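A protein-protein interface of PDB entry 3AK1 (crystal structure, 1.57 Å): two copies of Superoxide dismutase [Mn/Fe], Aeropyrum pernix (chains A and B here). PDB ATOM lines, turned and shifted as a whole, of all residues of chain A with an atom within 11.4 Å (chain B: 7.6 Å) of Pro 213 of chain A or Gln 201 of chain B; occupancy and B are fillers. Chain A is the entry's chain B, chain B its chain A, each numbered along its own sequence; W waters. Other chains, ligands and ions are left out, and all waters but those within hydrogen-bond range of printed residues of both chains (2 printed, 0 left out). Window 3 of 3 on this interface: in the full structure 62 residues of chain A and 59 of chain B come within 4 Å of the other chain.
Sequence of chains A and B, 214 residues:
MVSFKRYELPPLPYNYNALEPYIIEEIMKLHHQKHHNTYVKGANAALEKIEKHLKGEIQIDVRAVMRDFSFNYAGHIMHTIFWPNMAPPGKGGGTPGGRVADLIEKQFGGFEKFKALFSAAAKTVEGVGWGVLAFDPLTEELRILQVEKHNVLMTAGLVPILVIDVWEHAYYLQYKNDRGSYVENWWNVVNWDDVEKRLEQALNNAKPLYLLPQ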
ATOM      1  N   PRO A 137      21.191 -14.217  27.129  1.00  0.00           N
ATOM      2  CA  PRO A 137      20.461 -13.078  26.578  1.00  0.00           C
ATOM      3  C   PRO A 137      19.254 -12.642  27.419  1.00  0.00           C
ATOM      4  O   PRO A 137      18.833 -11.492  27.316  1.00  0.00           O
ATOM      5  CB  PRO A 137      20.012 -13.580  25.205  1.00  0.00           C
ATOM      6  CG  PRO A 137      19.942 -15.073  25.350  1.00  0.00           C
ATOM      7  CD  PRO A 137      21.108 -15.404  26.255  1.00  0.00           C
ATOM      8  N   GLU A 140      21.265 -11.054  30.705  1.00  0.00           N
ATOM      9  CA  GLU A 140      22.514 -10.340  30.396  1.00  0.00           C
ATOM     10  C   GLU A 140      23.611 -10.614  31.432  1.00  0.00           C
ATOM     11  O   GLU A 140      24.408  -9.733  31.786  1.00  0.00           O
ATOM     12  CB  GLU A 140      22.257  -8.844  30.155  1.00  0.00           C
ATOM     13  CG  GLU A 140      21.234  -8.619  29.044  1.00  0.00           C
ATOM     14  CD  GLU A 140      21.246  -7.222  28.463  1.00  0.00           C
ATOM     15  OE1 GLU A 140      21.821  -7.029  27.371  1.00  0.00           O
ATOM     16  OE2 GLU A 140      20.667  -6.318  29.085  1.00  0.00           O
ATOM     17  N   GLN A 201      30.021  -7.649  22.003  1.00  0.00           N
ATOM     18  CA  GLN A 201      29.031  -7.900  20.961  1.00  0.00           C
ATOM     19  C   GLN A 201      27.766  -8.518  21.551  1.00  0.00           C
ATOM     20  O   GLN A 201      26.657  -8.122  21.178  1.00  0.00           O
ATOM     21  CB  GLN A 201      29.603  -8.787  19.853  1.00  0.00           C
ATOM     22  CG  GLN A 201      30.799  -8.179  19.114  1.00  0.00           C
ATOM     23  CD  GLN A 201      30.460  -6.939  18.293  1.00  0.00           C
ATOM     24  OE1 GLN A 201      31.277  -6.017  18.182  1.00  0.00           O
ATOM     25  NE2 GLN A 201      29.266  -6.911  17.709  1.00  0.00           N
ATOM     26  N   ALA A 202      27.937  -9.457  22.486  1.00  0.00           N
ATOM     27  CA  ALA A 202      26.795 -10.084  23.173  1.00  0.00           C
ATOM     28  C   ALA A 202      25.946  -9.069  23.938  1.00  0.00           C
ATOM     29  O   ALA A 202      24.721  -9.054  23.815  1.00  0.00           O
ATOM     30  CB  ALA A 202      27.264 -11.216  24.095  1.00  0.00           C
ATOM     31  N   LEU A 203      26.606  -8.211  24.713  1.00  0.00           N
ATOM     32  CA  LEU A 203      25.926  -7.144  25.436  1.00  0.00           C
ATOM     33  C   LEU A 203      25.102  -6.269  24.503  1.00  0.00           C
ATOM     34  O   LEU A 203      24.015  -5.814  24.871  1.00  0.00           O
ATOM     35  CB  LEU A 203      26.928  -6.279  26.197  1.00  0.00           C
ATOM     36  CG  LEU A 203      27.434  -6.822  27.534  1.00  0.00           C
ATOM     37  CD1 LEU A 203      28.637  -6.033  27.983  1.00  0.00           C
ATOM     38  CD2 LEU A 203      26.339  -6.791  28.593  1.00  0.00           C
ATOM     39  N   ASN A 204      25.608  -6.043  23.294  1.00  0.00           N
ATOM     40  CA  ASN A 204      24.914  -5.184  22.337  1.00  0.00           C
ATOM     41  C   ASN A 204      23.846  -5.880  21.500  1.00  0.00           C
ATOM     42  O   ASN A 204      22.824  -5.264  21.170  1.00  0.00           O
ATOM     43  CB  ASN A 204      25.920  -4.467  21.440  1.00  0.00           C
ATOM     44  CG  ASN A 204      26.718  -3.420  22.192  1.00  0.00           C
ATOM     45  OD1 ASN A 204      26.207  -2.774  23.111  1.00  0.00           O
ATOM     46  ND2 ASN A 204      27.975  -3.246  21.806  1.00  0.00           N
ATOM     47  N   ASN A 205      24.069  -7.161  21.195  1.00  0.00           N
ATOM     48  CA  ASN A 205      23.302  -7.886  20.173  1.00  0.00           C
ATOM     49  C   ASN A 205      22.393  -9.031  20.622  1.00  0.00           C
ATOM     50  O   ASN A 205      21.427  -9.345  19.925  1.00  0.00           O
ATOM     51  CB  ASN A 205      24.251  -8.437  19.102  1.00  0.00           C
ATOM     52  CG  ASN A 205      24.902  -7.343  18.271  1.00  0.00           C
ATOM     53  OD1 ASN A 205      25.447  -6.378  18.805  1.00  0.00           O
ATOM     54  ND2 ASN A 205      24.856  -7.497  16.956  1.00  0.00           N
ATOM     55  N   ALA A 206      22.708  -9.672  21.748  1.00  0.00           N
ATOM     56  CA  ALA A 206      22.087 -10.968  22.076  1.00  0.00           C
ATOM     57  C   ALA A 206      20.630 -10.877  22.539  1.00  0.00           C
ATOM     58  O   ALA A 206      19.778 -11.615  22.056  1.00  0.00           O
ATOM     59  CB  ALA A 206      22.928 -11.737  23.093  1.00  0.00           C
ATOM     60  N   LYS A 207      20.351  -9.983  23.476  1.00  0.00           N
ATOM     61  CA  LYS A 207      19.008  -9.859  24.037  1.00  0.00           C
ATOM     62  C   LYS A 207      17.898  -9.662  22.980  1.00  0.00           C
ATOM     63  O   LYS A 207      16.910 -10.389  23.011  1.00  0.00           O
ATOM     64  CB  LYS A 207      18.962  -8.769  25.112  1.00  0.00           C
ATOM     65  CG  LYS A 207      17.643  -8.684  25.860  1.00  0.00           C
ATOM     66  CD  LYS A 207      17.799  -7.828  27.103  1.00  0.00           C
ATOM     67  CE  LYS A 207      16.464  -7.314  27.599  1.00  0.00           C
ATOM     68  NZ  LYS A 207      16.648  -6.451  28.809  1.00  0.00           N
ATOM     69  N   PRO A 208      18.059  -8.701  22.046  1.00  0.00           N
ATOM     70  CA  PRO A 208      17.003  -8.486  21.029  1.00  0.00           C
ATOM     71  C   PRO A 208      16.635  -9.694  20.143  1.00  0.00           C
ATOM     72  O   PRO A 208      15.553  -9.705  19.552  1.00  0.00           O
ATOM     73  CB  PRO A 208      17.577  -7.361  20.162  1.00  0.00           C
ATOM     74  CG  PRO A 208      18.555  -6.665  21.027  1.00  0.00           C
ATOM     75  CD  PRO A 208      19.165  -7.740  21.875  1.00  0.00           C
ATOM     76  N   LEU A 209      17.516 -10.688  20.046  1.00  0.00           N
ATOM     77  CA  LEU A 209      17.235 -11.898  19.273  1.00  0.00           C
ATOM     78  C   LEU A 209      16.050 -12.689  19.825  1.00  0.00           C
ATOM     79  O   LEU A 209      15.406 -13.445  19.092  1.00  0.00           O
ATOM     80  CB  LEU A 209      18.467 -12.812  19.237  1.00  0.00           C
ATOM     81  CG  LEU A 209      19.732 -12.324  18.535  1.00  0.00           C
ATOM     82  CD1 LEU A 209      20.879 -13.287  18.781  1.00  0.00           C
ATOM     83  CD2 LEU A 209      19.477 -12.191  17.052  1.00  0.00           C
ATOM     84  N   TYR A 210      15.777 -12.521  21.121  1.00  0.00           N
ATOM     85  CA  TYR A 210      14.801 -13.360  21.825  1.00  0.00           C
ATOM     86  C   TYR A 210      13.672 -12.579  22.474  1.00  0.00           C
ATOM     87  O   TYR A 210      12.517 -13.013  22.475  1.00  0.00           O
ATOM     88  CB  TYR A 210      15.518 -14.212  22.868  1.00  0.00           C
ATOM     89  CG  TYR A 210      16.531 -15.111  22.223  1.00  0.00           C
ATOM     90  CD1 TYR A 210      16.127 -16.259  21.551  1.00  0.00           C
ATOM     91  CD2 TYR A 210      17.888 -14.800  22.245  1.00  0.00           C
ATOM     92  CE1 TYR A 210      17.041 -17.086  20.934  1.00  0.00           C
ATOM     93  CE2 TYR A 210      18.819 -15.628  21.628  1.00  0.00           C
ATOM     94  CZ  TYR A 210      18.382 -16.771  20.967  1.00  0.00           C
ATOM     95  OH  TYR A 210      19.272 -17.617  20.346  1.00  0.00           O
ATOM     96  N   LEU A 211      14.025 -11.440  23.052  1.00  0.00           N
ATOM     97  CA  LEU A 211      13.048 -10.534  23.617  1.00  0.00           C
ATOM     98  C   LEU A 211      12.989  -9.347  22.665  1.00  0.00           C
ATOM     99  O   LEU A 211      13.897  -8.506  22.642  1.00  0.00           O
ATOM    100  CB  LEU A 211      13.440 -10.137  25.052  1.00  0.00           C
ATOM    101  CG  LEU A 211      13.795 -11.286  26.018  1.00  0.00           C
ATOM    102  CD1 LEU A 211      14.283 -10.766  27.376  1.00  0.00           C
ATOM    103  CD2 LEU A 211      12.624 -12.269  26.196  1.00  0.00           C
ATOM    104  N   LEU A 212      11.928  -9.322  21.858  1.00  0.00           N
ATOM    105  CA  LEU A 212      11.789  -8.383  20.745  1.00  0.00           C
ATOM    106  C   LEU A 212      11.594  -6.939  21.205  1.00  0.00           C
ATOM    107  O   LEU A 212      10.762  -6.674  22.071  1.00  0.00           O
ATOM    108  CB  LEU A 212      10.633  -8.797  19.821  1.00  0.00           C
ATOM    109  CG  LEU A 212      10.729 -10.117  19.036  1.00  0.00           C
ATOM    110  CD1 LEU A 212       9.412 -10.448  18.345  1.00  0.00           C
ATOM    111  CD2 LEU A 212      11.870 -10.088  18.028  1.00  0.00           C
ATOM    112  N   PRO A 213      12.367  -6.004  20.621  1.00  0.00           N
ATOM    113  CA  PRO A 213      12.250  -4.587  20.942  1.00  0.00           C
ATOM    114  C   PRO A 213      11.284  -3.874  19.995  1.00  0.00           C
ATOM    115  O   PRO A 213      10.071  -4.081  20.087  1.00  0.00           O
ATOM    116  CB  PRO A 213      13.680  -4.072  20.748  1.00  0.00           C
ATOM    117  CG  PRO A 213      14.299  -5.008  19.713  1.00  0.00           C
ATOM    118  CD  PRO A 213      13.417  -6.246  19.612  1.00  0.00           C
ATOM    119  N   PHE B 135      17.990 -19.539  12.499  1.00  0.00           N
ATOM    120  CA  PHE B 135      18.884 -18.715  11.701  1.00  0.00           C
ATOM    121  C   PHE B 135      20.329 -19.053  12.051  1.00  0.00           C
ATOM    122  O   PHE B 135      20.707 -19.025  13.218  1.00  0.00           O
ATOM    123  CB  PHE B 135      18.612 -17.230  11.966  1.00  0.00           C
ATOM    124  CG  PHE B 135      19.410 -16.298  11.097  1.00  0.00           C
ATOM    125  CD1 PHE B 135      18.976 -15.985   9.811  1.00  0.00           C
ATOM    126  CD2 PHE B 135      20.593 -15.727  11.560  1.00  0.00           C
ATOM    127  CE1 PHE B 135      19.703 -15.116   8.996  1.00  0.00           C
ATOM    128  CE2 PHE B 135      21.321 -14.866  10.755  1.00  0.00           C
ATOM    129  CZ  PHE B 135      20.875 -14.560   9.468  1.00  0.00           C
ATOM    130  N   VAL B 159      19.963 -19.672  15.921  1.00  0.00           N
ATOM    131  CA  VAL B 159      18.945 -18.873  16.589  1.00  0.00           C
ATOM    132  C   VAL B 159      17.539 -19.375  16.221  1.00  0.00           C
ATOM    133  O   VAL B 159      17.082 -19.175  15.084  1.00  0.00           O
ATOM    134  CB  VAL B 159      19.078 -17.357  16.232  1.00  0.00           C
ATOM    135  CG1 VAL B 159      18.085 -16.534  17.052  1.00  0.00           C
ATOM    136  CG2 VAL B 159      20.520 -16.857  16.446  1.00  0.00           C
ATOM    137  N   ILE B 161      13.947 -19.230  15.432  1.00  0.00           N
ATOM    138  CA  ILE B 161      12.951 -18.204  15.093  1.00  0.00           C
ATOM    139  C   ILE B 161      11.524 -18.775  15.049  1.00  0.00           C
ATOM    140  O   ILE B 161      10.537 -18.034  15.138  1.00  0.00           O
ATOM    141  CB  ILE B 161      13.278 -17.474  13.760  1.00  0.00           C
ATOM    142  CG1 ILE B 161      13.338 -18.454  12.576  1.00  0.00           C
ATOM    143  CG2 ILE B 161      14.585 -16.692  13.891  1.00  0.00           C
ATOM    144  CD1 ILE B 161      13.303 -17.783  11.183  1.00  0.00           C
ATOM    145  N   VAL B 195       7.571 -14.547  13.655  1.00  0.00           N
ATOM    146  CA  VAL B 195       8.717 -15.190  13.007  1.00  0.00           C
ATOM    147  C   VAL B 195       9.514 -14.180  12.162  1.00  0.00           C
ATOM    148  O   VAL B 195      10.741 -14.181  12.173  1.00  0.00           O
ATOM    149  CB  VAL B 195       8.261 -16.406  12.147  1.00  0.00           C
ATOM    150  CG1 VAL B 195       9.444 -17.095  11.487  1.00  0.00           C
ATOM    151  CG2 VAL B 195       7.445 -17.408  12.993  1.00  0.00           C
ATOM    152  N   GLU B 196       8.807 -13.310  11.442  1.00  0.00           N
ATOM    153  CA  GLU B 196       9.435 -12.300  10.594  1.00  0.00           C
ATOM    154  C   GLU B 196      10.251 -11.333  11.442  1.00  0.00           C
ATOM    155  O   GLU B 196      11.383 -10.971  11.092  1.00  0.00           O
ATOM    156  CB  GLU B 196       8.365 -11.552   9.780  1.00  0.00           C
ATOM    157  CG  GLU B 196       8.899 -10.457   8.837  1.00  0.00           C
ATOM    158  CD  GLU B 196       9.690 -10.992   7.646  1.00  0.00           C
ATOM    159  OE1 GLU B 196       9.541 -12.184   7.293  1.00  0.00           O
ATOM    160  OE2 GLU B 196      10.461 -10.202   7.048  1.00  0.00           O
ATOM    161  N   LYS B 197       9.668 -10.928  12.569  1.00  0.00           N
ATOM    162  CA  LYS B 197      10.332 -10.029  13.504  1.00  0.00           C
ATOM    163  C   LYS B 197      11.571 -10.678  14.107  1.00  0.00           C
ATOM    164  O   LYS B 197      12.600 -10.018  14.287  1.00  0.00           O
ATOM    165  CB  LYS B 197       9.370  -9.575  14.599  1.00  0.00           C
ATOM    166  CG  LYS B 197       8.412  -8.468  14.160  1.00  0.00           C
ATOM    167  CD  LYS B 197       7.289  -8.287  15.177  1.00  0.00           C
ATOM    168  CE  LYS B 197       6.511  -6.998  14.947  1.00  0.00           C
ATOM    169  NZ  LYS B 197       5.826  -6.978  13.618  1.00  0.00           N
ATOM    170  N   ARG B 198      11.485 -11.975  14.390  1.00  0.00           N
ATOM    171  CA  ARG B 198      12.645 -12.702  14.905  1.00  0.00           C
ATOM    172  C   ARG B 198      13.726 -12.793  13.849  1.00  0.00           C
ATOM    173  O   ARG B 198      14.900 -12.575  14.145  1.00  0.00           O
ATOM    174  CB  ARG B 198      12.261 -14.091  15.430  1.00  0.00           C
ATOM    175  CG  ARG B 198      11.520 -14.009  16.749  1.00  0.00           C
ATOM    176  CD  ARG B 198      11.036 -15.363  17.277  1.00  0.00           C
ATOM    177  NE  ARG B 198      10.073 -15.099  18.336  1.00  0.00           N
ATOM    178  CZ  ARG B 198      10.384 -14.761  19.581  1.00  0.00           C
ATOM    179  NH1 ARG B 198      11.648 -14.720  19.970  1.00  0.00           N
ATOM    180  NH2 ARG B 198       9.420 -14.494  20.448  1.00  0.00           N
ATOM    181  N   LEU B 199      13.330 -13.085  12.612  1.00  0.00           N
ATOM    182  CA  LEU B 199      14.295 -13.160  11.524  1.00  0.00           C
ATOM    183  C   LEU B 199      14.994 -11.822  11.298  1.00  0.00           C
ATOM    184  O   LEU B 199      16.201 -11.796  11.066  1.00  0.00           O
ATOM    185  CB  LEU B 199      13.648 -13.668  10.237  1.00  0.00           C
ATOM    186  CG  LEU B 199      14.582 -13.691   9.024  1.00  0.00           C
ATOM    187  CD1 LEU B 199      15.772 -14.627   9.198  1.00  0.00           C
ATOM    188  CD2 LEU B 199      13.808 -14.040   7.778  1.00  0.00           C
ATOM    189  N   GLU B 200      14.246 -10.722  11.379  1.00  0.00           N
ATOM    190  CA  GLU B 200      14.855  -9.405  11.145  1.00  0.00           C
ATOM    191  C   GLU B 200      15.914  -9.065  12.205  1.00  0.00           C
ATOM    192  O   GLU B 200      16.998  -8.593  11.863  1.00  0.00           O
ATOM    193  CB  GLU B 200      13.808  -8.294  10.910  1.00  0.00           C
ATOM    194  CG  GLU B 200      12.870  -7.998  12.059  1.00  0.00           C
ATOM    195  CD  GLU B 200      11.814  -6.920  11.743  1.00  0.00           C
ATOM    196  OE1 GLU B 200      11.084  -7.041  10.723  1.00  0.00           O
ATOM    197  OE2 GLU B 200      11.706  -5.955  12.536  1.00  0.00           O
ATOM    198  N   GLN B 201      15.635  -9.395  13.469  1.00  0.00           N
ATOM    199  CA  GLN B 201      16.619  -9.245  14.545  1.00  0.00           C
ATOM    200  C   GLN B 201      17.868 -10.089  14.289  1.00  0.00           C
ATOM    201  O   GLN B 201      18.993  -9.605  14.440  1.00  0.00           O
ATOM    202  CB  GLN B 201      16.015  -9.584  15.917  1.00  0.00           C
ATOM    203  CG  GLN B 201      14.968  -8.594  16.401  1.00  0.00           C
ATOM    204  CD  GLN B 201      15.437  -7.147  16.281  1.00  0.00           C
ATOM    205  OE1 GLN B 201      16.410  -6.740  16.916  1.00  0.00           O
ATOM    206  NE2 GLN B 201      14.742  -6.367  15.462  1.00  0.00           N
ATOM    207  N   ALA B 202      17.663 -11.340  13.884  1.00  0.00           N
ATOM    208  CA  ALA B 202      18.765 -12.266  13.627  1.00  0.00           C
ATOM    209  C   ALA B 202      19.636 -11.790  12.466  1.00  0.00           C
ATOM    210  O   ALA B 202      20.869 -11.837  12.540  1.00  0.00           O
ATOM    211  CB  ALA B 202      18.232 -13.673  13.374  1.00  0.00           C
ATOM    212  N   LEU B 203      18.985 -11.318  11.405  1.00  0.00           N
ATOM    213  CA  LEU B 203      19.680 -10.770  10.244  1.00  0.00           C
ATOM    214  C   LEU B 203      20.597  -9.609  10.602  1.00  0.00           C
ATOM    215  O   LEU B 203      21.678  -9.485  10.022  1.00  0.00           O
ATOM    216  CB  LEU B 203      18.681 -10.333   9.174  1.00  0.00           C
ATOM    217  CG  LEU B 203      18.084 -11.447   8.320  1.00  0.00           C
ATOM    218  CD1 LEU B 203      16.809 -10.950   7.676  1.00  0.00           C
ATOM    219  CD2 LEU B 203      19.090 -11.931   7.278  1.00  0.00           C
ATOM    220  N   ASN B 204      20.161  -8.771  11.545  1.00  0.00           N
ATOM    221  CA  ASN B 204      20.952  -7.628  12.014  1.00  0.00           C
ATOM    222  C   ASN B 204      22.001  -7.996  13.054  1.00  0.00           C
ATOM    223  O   ASN B 204      23.080  -7.399  13.082  1.00  0.00           O
ATOM    224  CB  ASN B 204      20.059  -6.532  12.611  1.00  0.00           C
ATOM    225  CG  ASN B 204      19.041  -5.973  11.621  1.00  0.00           C
ATOM    226  OD1 ASN B 204      17.955  -5.545  12.019  1.00  0.00           O
ATOM    227  ND2 ASN B 204      19.385  -5.966  10.335  1.00  0.00           N
ATOM    228  N   ASN B 205      21.691  -8.970  13.911  1.00  0.00           N
ATOM    229  CA  ASN B 205      22.465  -9.158  15.145  1.00  0.00           C
ATOM    230  C   ASN B 205      23.313 -10.424  15.297  1.00  0.00           C
ATOM    231  O   ASN B 205      24.273 -10.418  16.055  1.00  0.00           O
ATOM    232  CB  ASN B 205      21.550  -9.016  16.372  1.00  0.00           C
ATOM    233  CG  ASN B 205      21.152  -7.570  16.652  1.00  0.00           C
ATOM    234  OD1 ASN B 205      21.009  -6.756  15.739  1.00  0.00           O
ATOM    235  ND2 ASN B 205      20.955  -7.256  17.919  1.00  0.00           N
ATOM    236  N   ALA B 206      22.956 -11.503  14.602  1.00  0.00           N
ATOM    237  CA  ALA B 206      23.523 -12.824  14.905  1.00  0.00           C
ATOM    238  C   ALA B 206      24.990 -13.017  14.518  1.00  0.00           C
ATOM    239  O   ALA B 206      25.792 -13.456  15.341  1.00  0.00           O
ATOM    240  CB  ALA B 206      22.669 -13.921  14.304  1.00  0.00           C
ATOM    241  N   LYS B 207      25.342 -12.693  13.277  1.00  0.00           N
ATOM    242  CA  LYS B 207      26.711 -12.915  12.795  1.00  0.00           C
ATOM    243  C   LYS B 207      27.815 -12.292  13.680  1.00  0.00           C
ATOM    244  O   LYS B 207      28.782 -12.990  14.015  1.00  0.00           O
ATOM    245  CB  LYS B 207      26.867 -12.528  11.316  1.00  0.00           C
ATOM    246  CG  LYS B 207      28.191 -12.998  10.699  1.00  0.00           C
ATOM    247  CD  LYS B 207      28.201 -12.863   9.180  1.00  0.00           C
ATOM    248  CE  LYS B 207      29.529 -13.352   8.606  1.00  0.00           C
ATOM    249  NZ  LYS B 207      29.618 -13.194   7.124  1.00  0.00           N
HETATM  250  O   HOH W   1      14.124 -15.841  18.669  1.00  0.00           O
HETATM  251  O   HOH W   2      15.873 -13.961  16.356  1.00  0.00           O
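The backbone carbonyl oxygen (O) of Tyr 210 of chain A sits at hydrogen-bond distance from the guanidinium group (NH1) of Arg 198 of chain B (3.2 Å). ND2 of Asn 205 of chain B sits at hydrogen-bond distance from O of Asn 205 of chain A (2.9 Å).
O of Val 159 of chain B sits at hydrogen-bond distance from N of Phe 135 of chain B (2.8 Å). The backbone carbonyl oxygen (O) of Gln 201 of chain A sits close to the side-chain amide oxygen (OD1) of Asn 205 of chain A (3.2 Å).
O of Pro 208 of chain A touches CG of Gln 201 of chain B, at 3.4 Å. ND2 of Asn 205 of chain B touches CG of Pro 208 of chain A (3.97 Å). Gln 201 of chain B touches Leu 209 of chain A (O to CD2, 3.7 Å). Ala 202 of chain B touches Leu 209 of chain A. CB of Asn 205 of chain B touches CD2 of Leu 209 of chain A (3.9 Å). Val 159 of chain B touches Tyr 210 of chain A (CG1 to OH, 3.7 Å). Leu 212 of chain A touches Lys 197 of chain B. Leu 212 of chain A touches Gln 201 of chain B. CG of Pro 213 of chain A touches OE1 of Gln 201 of chain B (3.9 Å).
Pro 213 of chain A touches just one residue of chain B: Gln 201 (3.9 Å). Gln 201 of chain B touches four residues of chain A. Of chain A, only Leu 209 comes within 4 Å of Ala 202 of chain B. No residue of chain A comes within 4 Å of Asn 204 of chain B. Asn 205 of chain B touches three residues of chain A. Of the printed residues of chain B, Leu 212 of chain A touches Lys 197 (3.8 Å) and Gln 201 (3.8 Å). Printed residues of chain A within 4 Å of Arg 198 of chain B: Tyr 210. Printed residues of chain A within 4 Å of Val 159 of chain B: Tyr 210 (3.7 Å). Of the printed residues of chain B, Asn 205 of chain A touches Asn 205. Leu 203 of chain A touches none of the printed residues of chain B. Leu 203 of chain B touches none of the printed residues of chain A. The nearest printed residue of chain B that does not touch Asn 205 of chain A is Asn 204 of chain B (4.3 Å).
Hydrophobic or aromatic side chains of chain B within 4 Å of the printed part of chain A: Val 159. Hydrophobic or aromatic side chains of chain A within 4 Å of the printed part of chain B: Pro 208, Leu 209, Tyr 210, Leu 212 and Pro 213. Among the printed residues, no Asp or Glu carboxylate lies within 4 Å of a Lys or Arg side-chain nitrogen of the other chain.
Asn 205 of chain B touches its own counterpart, Asn 205 of chain A. 7 positions are printed for both chains.
Water W1 bridges the backbone carbonyl oxygen (O) of Leu 209 of chain A (2.8 Å) and the guanidinium group (NH1) of Arg 198 of chain B (3.0 Å). Water W2 lies within hydrogen-bond range of O of Arg 198 of chain B (2.8 Å) and O of Leu 209 of chain A (2.8 Å).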
